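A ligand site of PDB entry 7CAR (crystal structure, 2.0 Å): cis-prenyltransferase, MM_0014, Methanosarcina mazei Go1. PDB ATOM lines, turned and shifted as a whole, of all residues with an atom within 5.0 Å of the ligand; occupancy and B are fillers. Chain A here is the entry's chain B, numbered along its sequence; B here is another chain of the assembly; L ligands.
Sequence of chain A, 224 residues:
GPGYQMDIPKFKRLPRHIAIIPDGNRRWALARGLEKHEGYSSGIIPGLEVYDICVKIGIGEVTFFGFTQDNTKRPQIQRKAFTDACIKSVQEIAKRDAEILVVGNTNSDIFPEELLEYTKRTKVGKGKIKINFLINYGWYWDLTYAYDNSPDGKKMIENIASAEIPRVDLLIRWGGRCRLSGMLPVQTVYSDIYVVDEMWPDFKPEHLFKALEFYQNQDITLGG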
ATOM      1  N   ILE A  21      -7.875 -11.592  -8.667  1.00  0.00           N
ATOM      2  CA  ILE A  21      -6.968 -12.354  -9.568  1.00  0.00           C
ATOM      3  C   ILE A  21      -7.663 -13.687  -9.801  1.00  0.00           C
ATOM      4  O   ILE A  21      -7.610 -14.587  -8.962  1.00  0.00           O
ATOM      5  CB  ILE A  21      -5.519 -12.486  -9.009  1.00  0.00           C
ATOM      6  CG1 ILE A  21      -4.894 -11.112  -8.737  1.00  0.00           C
ATOM      7  CG2 ILE A  21      -4.679 -13.264  -9.989  1.00  0.00           C
ATOM      8  CD1 ILE A  21      -3.418 -11.132  -8.283  1.00  0.00           C
ATOM      9  N   PRO A  22      -8.369 -13.834 -10.950  1.00  0.00           N
ATOM     10  CA  PRO A  22      -9.196 -15.004 -11.233  1.00  0.00           C
ATOM     11  C   PRO A  22      -8.382 -16.126 -11.877  1.00  0.00           C
ATOM     12  O   PRO A  22      -8.576 -16.458 -13.071  1.00  0.00           O
ATOM     13  CB  PRO A  22     -10.195 -14.373 -12.212  1.00  0.00           C
ATOM     14  CG  PRO A  22      -9.327 -13.516 -13.073  1.00  0.00           C
ATOM     15  CD  PRO A  22      -8.364 -12.890 -12.076  1.00  0.00           C
ATOM     16  N   ASP A  23      -7.439 -16.666 -11.115  1.00  0.00           N
ATOM     17  CA  ASP A  23      -6.409 -17.629 -11.569  1.00  0.00           C
ATOM     18  C   ASP A  23      -6.922 -19.053 -11.329  1.00  0.00           C
ATOM     19  O   ASP A  23      -7.854 -19.183 -10.529  1.00  0.00           O
ATOM     20  CB  ASP A  23      -5.083 -17.345 -10.836  1.00  0.00           C
ATOM     21  CG  ASP A  23      -3.889 -17.903 -11.579  1.00  0.00           C
ATOM     22  OD1 ASP A  23      -3.959 -17.926 -12.860  1.00  0.00           O
ATOM     23  OD2 ASP A  23      -2.973 -18.409 -10.877  1.00  0.00           O
ATOM     24  N   ASN A  25      -7.599 -21.354 -13.980  1.00  0.00           N
ATOM     25  CA  ASN A  25      -8.460 -21.776 -15.123  1.00  0.00           C
ATOM     26  C   ASN A  25      -7.868 -23.004 -15.850  1.00  0.00           C
ATOM     27  O   ASN A  25      -8.626 -23.939 -16.138  1.00  0.00           O
ATOM     28  CB  ASN A  25      -8.618 -20.623 -16.095  1.00  0.00           C
ATOM     29  CG  ASN A  25      -9.256 -19.436 -15.428  1.00  0.00           C
ATOM     30  OD1 ASN A  25     -10.402 -19.466 -15.058  1.00  0.00           O
ATOM     31  ND2 ASN A  25      -8.526 -18.386 -15.204  1.00  0.00           N
ATOM     32  N   TYR A  40     -10.914 -21.181 -19.432  1.00  0.00           N
ATOM     33  CA  TYR A  40     -11.053 -19.708 -19.397  1.00  0.00           C
ATOM     34  C   TYR A  40     -12.542 -19.331 -19.528  1.00  0.00           C
ATOM     35  O   TYR A  40     -13.031 -18.598 -18.676  1.00  0.00           O
ATOM     36  CB  TYR A  40     -10.140 -19.055 -20.442  1.00  0.00           C
ATOM     37  CG  TYR A  40      -8.667 -19.155 -20.127  1.00  0.00           C
ATOM     38  CD1 TYR A  40      -8.115 -18.575 -18.995  1.00  0.00           C
ATOM     39  CD2 TYR A  40      -7.802 -19.816 -20.985  1.00  0.00           C
ATOM     40  CE1 TYR A  40      -6.760 -18.671 -18.710  1.00  0.00           C
ATOM     41  CE2 TYR A  40      -6.439 -19.904 -20.720  1.00  0.00           C
ATOM     42  CZ  TYR A  40      -5.916 -19.338 -19.569  1.00  0.00           C
ATOM     43  OH  TYR A  40      -4.575 -19.433 -19.305  1.00  0.00           O
ATOM     44  N   GLY A  43     -14.683 -19.064 -16.706  1.00  0.00           N
ATOM     45  CA  GLY A  43     -14.319 -17.958 -15.798  1.00  0.00           C
ATOM     46  C   GLY A  43     -15.317 -16.814 -15.886  1.00  0.00           C
ATOM     47  O   GLY A  43     -15.281 -15.936 -14.998  1.00  0.00           O
ATOM     48  N   ILE A  44     -16.222 -16.817 -16.874  1.00  0.00           N
ATOM     49  CA  ILE A  44     -17.052 -15.609 -17.218  1.00  0.00           C
ATOM     50  C   ILE A  44     -18.146 -15.438 -16.150  1.00  0.00           C
ATOM     51  O   ILE A  44     -18.222 -14.373 -15.515  1.00  0.00           O
ATOM     52  CB  ILE A  44     -17.567 -15.697 -18.671  1.00  0.00           C
ATOM     53  CG1 ILE A  44     -16.424 -15.714 -19.680  1.00  0.00           C
ATOM     54  CG2 ILE A  44     -18.563 -14.580 -18.964  1.00  0.00           C
ATOM     55  CD1 ILE A  44     -16.830 -16.138 -21.088  1.00  0.00           C
ATOM     56  N   PHE A  64     -10.619  -6.274 -11.758  1.00  0.00           N
ATOM     57  CA  PHE A  64     -10.306  -7.609 -12.306  1.00  0.00           C
ATOM     58  C   PHE A  64      -8.952  -7.572 -13.020  1.00  0.00           C
ATOM     59  O   PHE A  64      -8.672  -6.690 -13.870  1.00  0.00           O
ATOM     60  CB  PHE A  64     -11.415  -8.121 -13.220  1.00  0.00           C
ATOM     61  CG  PHE A  64     -12.709  -8.418 -12.506  1.00  0.00           C
ATOM     62  CD1 PHE A  64     -12.915  -9.639 -11.875  1.00  0.00           C
ATOM     63  CD2 PHE A  64     -13.717  -7.476 -12.446  1.00  0.00           C
ATOM     64  CE1 PHE A  64     -14.107  -9.909 -11.238  1.00  0.00           C
ATOM     65  CE2 PHE A  64     -14.907  -7.751 -11.800  1.00  0.00           C
ATOM     66  CZ  PHE A  64     -15.101  -8.979 -11.207  1.00  0.00           C
ATOM     67  N   PHE A  65      -8.110  -8.529 -12.665  1.00  0.00           N
ATOM     68  CA  PHE A  65      -6.933  -8.918 -13.447  1.00  0.00           C
ATOM     69  C   PHE A  65      -7.490  -9.684 -14.659  1.00  0.00           C
ATOM     70  O   PHE A  65      -8.056 -10.760 -14.443  1.00  0.00           O
ATOM     71  CB  PHE A  65      -6.011  -9.703 -12.513  1.00  0.00           C
ATOM     72  CG  PHE A  65      -4.629  -9.971 -13.021  1.00  0.00           C
ATOM     73  CD1 PHE A  65      -4.385 -10.312 -14.337  1.00  0.00           C
ATOM     74  CD2 PHE A  65      -3.566  -9.967 -12.129  1.00  0.00           C
ATOM     75  CE1 PHE A  65      -3.095 -10.612 -14.762  1.00  0.00           C
ATOM     76  CE2 PHE A  65      -2.288 -10.270 -12.565  1.00  0.00           C
ATOM     77  CZ  PHE A  65      -2.061 -10.605 -13.864  1.00  0.00           C
ATOM     78  N   GLY A  66      -7.432  -9.104 -15.870  1.00  0.00           N
ATOM     79  CA  GLY A  66      -7.853  -9.810 -17.101  1.00  0.00           C
ATOM     80  C   GLY A  66      -6.723 -10.626 -17.673  1.00  0.00           C
ATOM     81  O   GLY A  66      -6.681 -11.870 -17.484  1.00  0.00           O
ATOM     82  N   THR A  68      -2.177  -9.930 -18.784  1.00  0.00           N
ATOM     83  CA  THR A  68      -0.968  -9.056 -18.801  1.00  0.00           C
ATOM     84  C   THR A  68      -0.163  -9.314 -20.059  1.00  0.00           C
ATOM     85  O   THR A  68      -0.409 -10.333 -20.702  1.00  0.00           O
ATOM     86  CB  THR A  68      -0.061  -9.333 -17.603  1.00  0.00           C
ATOM     87  OG1 THR A  68       0.296 -10.709 -17.627  1.00  0.00           O
ATOM     88  CG2 THR A  68      -0.747  -8.980 -16.312  1.00  0.00           C
ATOM     89  N   ASN A  71       1.362 -12.550 -19.862  1.00  0.00           N
ATOM     90  CA  ASN A  71       0.415 -13.662 -20.171  1.00  0.00           C
ATOM     91  C   ASN A  71       0.414 -13.970 -21.689  1.00  0.00           C
ATOM     92  O   ASN A  71       0.068 -15.113 -22.046  1.00  0.00           O
ATOM     93  CB  ASN A  71      -1.013 -13.341 -19.731  1.00  0.00           C
ATOM     94  CG  ASN A  71      -1.246 -13.428 -18.225  1.00  0.00           C
ATOM     95  OD1 ASN A  71      -0.507 -14.093 -17.491  1.00  0.00           O
ATOM     96  ND2 ASN A  71      -2.277 -12.740 -17.760  1.00  0.00           N
ATOM     97  N   ARG A  74       2.229 -17.001 -23.462  1.00  0.00           N
ATOM     98  CA  ARG A  74       1.617 -18.358 -23.369  1.00  0.00           C
ATOM     99  C   ARG A  74       1.183 -18.748 -24.790  1.00  0.00           C
ATOM    100  O   ARG A  74       1.053 -17.870 -25.643  1.00  0.00           O
ATOM    101  CB  ARG A  74       0.500 -18.357 -22.315  1.00  0.00           C
ATOM    102  CG  ARG A  74       0.998 -17.873 -20.955  1.00  0.00           C
ATOM    103  CD  ARG A  74       0.341 -18.499 -19.746  1.00  0.00           C
ATOM    104  NE  ARG A  74      -0.881 -17.785 -19.394  1.00  0.00           N
ATOM    105  CZ  ARG A  74      -1.283 -17.450 -18.164  1.00  0.00           C
ATOM    106  NH1 ARG A  74      -2.426 -16.814 -18.016  1.00  0.00           N
ATOM    107  NH2 ARG A  74      -0.545 -17.737 -17.110  1.00  0.00           N
ATOM    108  N   PHE A  82      -8.255 -16.875 -23.362  1.00  0.00           N
ATOM    109  CA  PHE A  82      -8.340 -15.939 -22.208  1.00  0.00           C
ATOM    110  C   PHE A  82      -8.740 -14.553 -22.735  1.00  0.00           C
ATOM    111  O   PHE A  82      -9.491 -13.851 -22.015  1.00  0.00           O
ATOM    112  CB  PHE A  82      -7.109 -15.954 -21.276  1.00  0.00           C
ATOM    113  CG  PHE A  82      -5.782 -15.440 -21.774  1.00  0.00           C
ATOM    114  CD1 PHE A  82      -5.587 -14.112 -22.127  1.00  0.00           C
ATOM    115  CD2 PHE A  82      -4.668 -16.280 -21.762  1.00  0.00           C
ATOM    116  CE1 PHE A  82      -4.333 -13.659 -22.535  1.00  0.00           C
ATOM    117  CE2 PHE A  82      -3.417 -15.832 -22.184  1.00  0.00           C
ATOM    118  CZ  PHE A  82      -3.248 -14.519 -22.563  1.00  0.00           C
ATOM    119  N   ALA A  85     -12.505 -14.607 -23.377  1.00  0.00           N
ATOM    120  CA  ALA A  85     -13.253 -14.666 -22.091  1.00  0.00           C
ATOM    121  C   ALA A  85     -13.245 -13.281 -21.431  1.00  0.00           C
ATOM    122  O   ALA A  85     -14.287 -12.872 -20.891  1.00  0.00           O
ATOM    123  CB  ALA A  85     -12.662 -15.741 -21.207  1.00  0.00           C
ATOM    124  N   CYS A  86     -12.104 -12.562 -21.494  1.00  0.00           N
ATOM    125  CA  CYS A  86     -11.979 -11.172 -20.991  1.00  0.00           C
ATOM    126  C   CYS A  86     -12.951 -10.274 -21.763  1.00  0.00           C
ATOM    127  O   CYS A  86     -13.803  -9.611 -21.129  1.00  0.00           O
ATOM    128  CB  CYS A  86     -10.540 -10.648 -21.082  1.00  0.00           C
ATOM    129  SG  CYS A  86      -9.445 -11.295 -19.775  1.00  0.00           S
ATOM    130  N   SER A  89     -16.514 -11.033 -20.657  1.00  0.00           N
ATOM    131  CA  SER A  89     -16.673 -10.533 -19.261  1.00  0.00           C
ATOM    132  C   SER A  89     -16.926  -9.021 -19.261  1.00  0.00           C
ATOM    133  O   SER A  89     -17.834  -8.566 -18.567  1.00  0.00           O
ATOM    134  CB  SER A  89     -15.485 -10.857 -18.420  1.00  0.00           C
ATOM    135  OG  SER A  89     -15.194 -12.244 -18.464  1.00  0.00           O
ATOM    136  N   PHE A 133     -10.834  -3.335 -15.428  1.00  0.00           N
ATOM    137  CA  PHE A 133     -10.217  -4.554 -16.019  1.00  0.00           C
ATOM    138  C   PHE A 133      -8.805  -4.193 -16.445  1.00  0.00           C
ATOM    139  O   PHE A 133      -8.594  -3.153 -17.099  1.00  0.00           O
ATOM    140  CB  PHE A 133     -11.026  -5.033 -17.230  1.00  0.00           C
ATOM    141  CG  PHE A 133     -12.458  -5.391 -16.923  1.00  0.00           C
ATOM    142  CD1 PHE A 133     -13.453  -4.431 -16.979  1.00  0.00           C
ATOM    143  CD2 PHE A 133     -12.798  -6.689 -16.596  1.00  0.00           C
ATOM    144  CE1 PHE A 133     -14.759  -4.759 -16.671  1.00  0.00           C
ATOM    145  CE2 PHE A 133     -14.106  -7.026 -16.292  1.00  0.00           C
ATOM    146  CZ  PHE A 133     -15.085  -6.058 -16.324  1.00  0.00           C
ATOM    147  N   ARG A 173      -7.206 -13.733  -4.597  1.00  0.00           N
ATOM    148  CA  ARG A 173      -6.613 -14.551  -5.671  1.00  0.00           C
ATOM    149  C   ARG A 173      -7.131 -15.977  -5.522  1.00  0.00           C
ATOM    150  O   ARG A 173      -6.933 -16.547  -4.491  1.00  0.00           O
ATOM    151  CB  ARG A 173      -5.085 -14.525  -5.603  1.00  0.00           C
ATOM    152  CG  ARG A 173      -4.411 -15.410  -6.641  1.00  0.00           C
ATOM    153  CD  ARG A 173      -3.019 -14.931  -6.973  1.00  0.00           C
ATOM    154  NE  ARG A 173      -2.476 -15.753  -8.043  1.00  0.00           N
ATOM    155  CZ  ARG A 173      -1.599 -15.353  -8.939  1.00  0.00           C
ATOM    156  NH1 ARG A 173      -1.092 -14.115  -8.901  1.00  0.00           N
ATOM    157  NH2 ARG A 173      -1.188 -16.222  -9.850  1.00  0.00           N
ATOM    158  N   ARG A 177      -2.181 -19.750  -5.407  1.00  0.00           N
ATOM    159  CA  ARG A 177      -0.835 -19.071  -5.378  1.00  0.00           C
ATOM    160  C   ARG A 177      -0.909 -17.737  -4.623  1.00  0.00           C
ATOM    161  O   ARG A 177      -1.812 -16.933  -4.866  1.00  0.00           O
ATOM    162  CB  ARG A 177      -0.312 -18.827  -6.795  1.00  0.00           C
ATOM    163  CG  ARG A 177      -0.319 -20.078  -7.668  1.00  0.00           C
ATOM    164  CD  ARG A 177       0.013 -19.770  -9.111  1.00  0.00           C
ATOM    165  NE  ARG A 177       1.410 -19.340  -9.198  1.00  0.00           N
ATOM    166  CZ  ARG A 177       2.040 -18.947 -10.284  1.00  0.00           C
ATOM    167  NH1 ARG A 177       1.413 -18.843 -11.452  1.00  0.00           N
ATOM    168  NH2 ARG A 177       3.313 -18.610 -10.191  1.00  0.00           N
ATOM    169  N   SER A 181       1.647 -11.354  -9.221  1.00  0.00           N
ATOM    170  CA  SER A 181       1.888 -11.532 -10.668  1.00  0.00           C
ATOM    171  C   SER A 181       1.871 -10.154 -11.343  1.00  0.00           C
ATOM    172  O   SER A 181       1.225 -10.014 -12.412  1.00  0.00           O
ATOM    173  CB  SER A 181       0.901 -12.505 -11.252  1.00  0.00           C
ATOM    174  OG  SER A 181       1.035 -13.826 -10.652  1.00  0.00           O
ATOM    175  N   TRP A 200     -10.428 -20.594 -10.043  1.00  0.00           N
ATOM    176  CA  TRP A 200     -11.414 -19.515 -10.310  1.00  0.00           C
ATOM    177  C   TRP A 200     -12.730 -20.087 -10.839  1.00  0.00           C
ATOM    178  O   TRP A 200     -13.786 -19.671 -10.382  1.00  0.00           O
ATOM    179  CB  TRP A 200     -10.816 -18.497 -11.252  1.00  0.00           C
ATOM    180  CG  TRP A 200     -11.754 -17.475 -11.799  1.00  0.00           C
ATOM    181  CD1 TRP A 200     -12.130 -17.305 -13.096  1.00  0.00           C
ATOM    182  CD2 TRP A 200     -12.441 -16.464 -11.046  1.00  0.00           C
ATOM    183  NE1 TRP A 200     -12.999 -16.244 -13.206  1.00  0.00           N
ATOM    184  CE2 TRP A 200     -13.200 -15.707 -11.967  1.00  0.00           C
ATOM    185  CE3 TRP A 200     -12.471 -16.107  -9.690  1.00  0.00           C
ATOM    186  CZ2 TRP A 200     -13.968 -14.615 -11.567  1.00  0.00           C
ATOM    187  CZ3 TRP A 200     -13.256 -15.049  -9.305  1.00  0.00           C
ATOM    188  CH2 TRP A 200     -13.985 -14.300 -10.223  1.00  0.00           C
ATOM    189  N   GLY B 224       4.366 -16.838 -14.510  1.00  0.00           N
ATOM    190  CA  GLY B 224       4.384 -15.744 -13.524  1.00  0.00           C
ATOM    191  C   GLY B 224       3.043 -15.540 -12.850  1.00  0.00           C
ATOM    192  O   GLY B 224       2.001 -15.969 -13.372  1.00  0.00           O
ATOM    193  OXT GLY B 224       2.993 -14.957 -11.773  1.00  0.00           O
HETATM  194  C1  LIG L   1      -0.962 -14.929 -13.462  1.00  0.00           C
HETATM  195  O1  LIG L   1      -0.359 -15.739 -12.695  1.00  0.00           O
HETATM  196  O2  LIG L   1      -0.442 -14.417 -14.488  1.00  0.00           O
HETATM  197  C2  LIG L   1      -2.394 -14.570 -13.126  1.00  0.00           C
HETATM  198  C3  LIG L   1      -3.382 -14.781 -14.208  1.00  0.00           C
HETATM  199  C4  LIG L   1      -4.740 -14.169 -13.868  1.00  0.00           C
HETATM  200  C5  LIG L   1      -5.621 -13.949 -15.052  1.00  0.00           C
HETATM  201  C6  LIG L   1      -5.823 -15.184 -15.874  1.00  0.00           C
HETATM  202  C7  LIG L   1      -7.256 -15.455 -16.230  1.00  0.00           C
HETATM  203  C8  LIG L   1      -7.689 -14.745 -17.479  1.00  0.00           C
HETATM  204  C9  LIG L   1      -9.102 -14.238 -17.442  1.00  0.00           C
HETATM  205  C10 LIG L   1     -10.115 -15.147 -18.104  1.00  0.00           C
HETATM  206  C11 LIG L   1     -11.110 -15.753 -17.150  1.00  0.00           C
HETATM  207  C12 LIG L   1     -12.381 -14.967 -17.025  1.00  0.00           C
HETATM  208  C13 LIG L   1     -12.212 -13.486 -16.807  1.00  0.00           C
HETATM  209  C14 LIG L   1     -12.951 -12.945 -15.607  1.00  0.00           C
HETATM  210  C15 LIG L   1     -12.427 -11.638 -15.099  1.00  0.00           C
HETATM  211  C16 LIG L   1     -11.928 -10.679 -16.160  1.00  0.00           C
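CG2 of Ile 21 touches C4 of the ligand, 3.98 Å away.
Pro 22 touches the ligand (O to C7, 3.6 Å).
Asp 23 touches the ligand (OD1 to C3, 3.5 Å).
Asn 25 touches the ligand.
Tyr 40 touches the ligand.
Gly 43 touches the ligand (C to C12, 3.7 Å).
Phe 64 touches the ligand (CD1 to C15, 3.8 Å).
CD1 of Phe 65 touches C4 of the ligand, at 3.9 Å.
Gly 66 touches the ligand.
Cys 86 touches the ligand.
Ser 89 touches the ligand.
16 residues have an atom within 4 Å of the ligand: Ile 21, Pro 22, Asp 23, Asn 25, Tyr 40, Gly 43, Phe 64, Phe 65, Gly 66, Asn 71, Cys 86, Ser 89, Arg 173, Arg 177, Ser 181 and Gly 224 of chain B.
O1 of the ligand lies within salt-bridge range of NH1 of Arg 177.
The side-chain amide oxygen (OD1) of Asn 71 lies close to an oxygen (O2) of the ligand (3.0 Å).
O of Gly 224 of chain B lies close to O1 of the ligand (2.5 Å).
The guanidinium group (NH2) of Arg 173 lies within salt-bridge range of an oxygen (O1) of the ligand (3.0 Å).
The side-chain hydroxyl (OG) of Ser 181 is in hydrogen-bond range of an oxygen (O1) of the ligand, 3.1 Å away.
The chain-end carboxylate (O) of Gly 224 of chain B lies within salt-bridge range of the guanidinium group (NH1) of Arg 177, 3.5 Å away.
OD1 of Asn 71 sits at hydrogen-bond distance from NH1 of Arg 74 (3.4 Å).
The guanidinium group of Arg 173 is in salt-bridge range of the side-chain carboxylate of Asp 23 (3.0 Å).
ND2 of Asn 71 sits close to N of Thr 68, 3.0 Å away.
The side-chain amide nitrogen of Asn 25 sits at hydrogen-bond distance from the backbone carbonyl oxygen of Pro 22, 2.9 Å away.
The side-chain sulfur of Cys 86 lies close to the backbone carbonyl oxygen of Gly 66 (3.6 Å).
OG of Ser 89 sits at hydrogen-bond distance from O of Ala 85.
The backbone carbonyl oxygen (O) of Arg 177 sits close to the guanidinium group (NE) of Arg 173 (3.5 Å).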
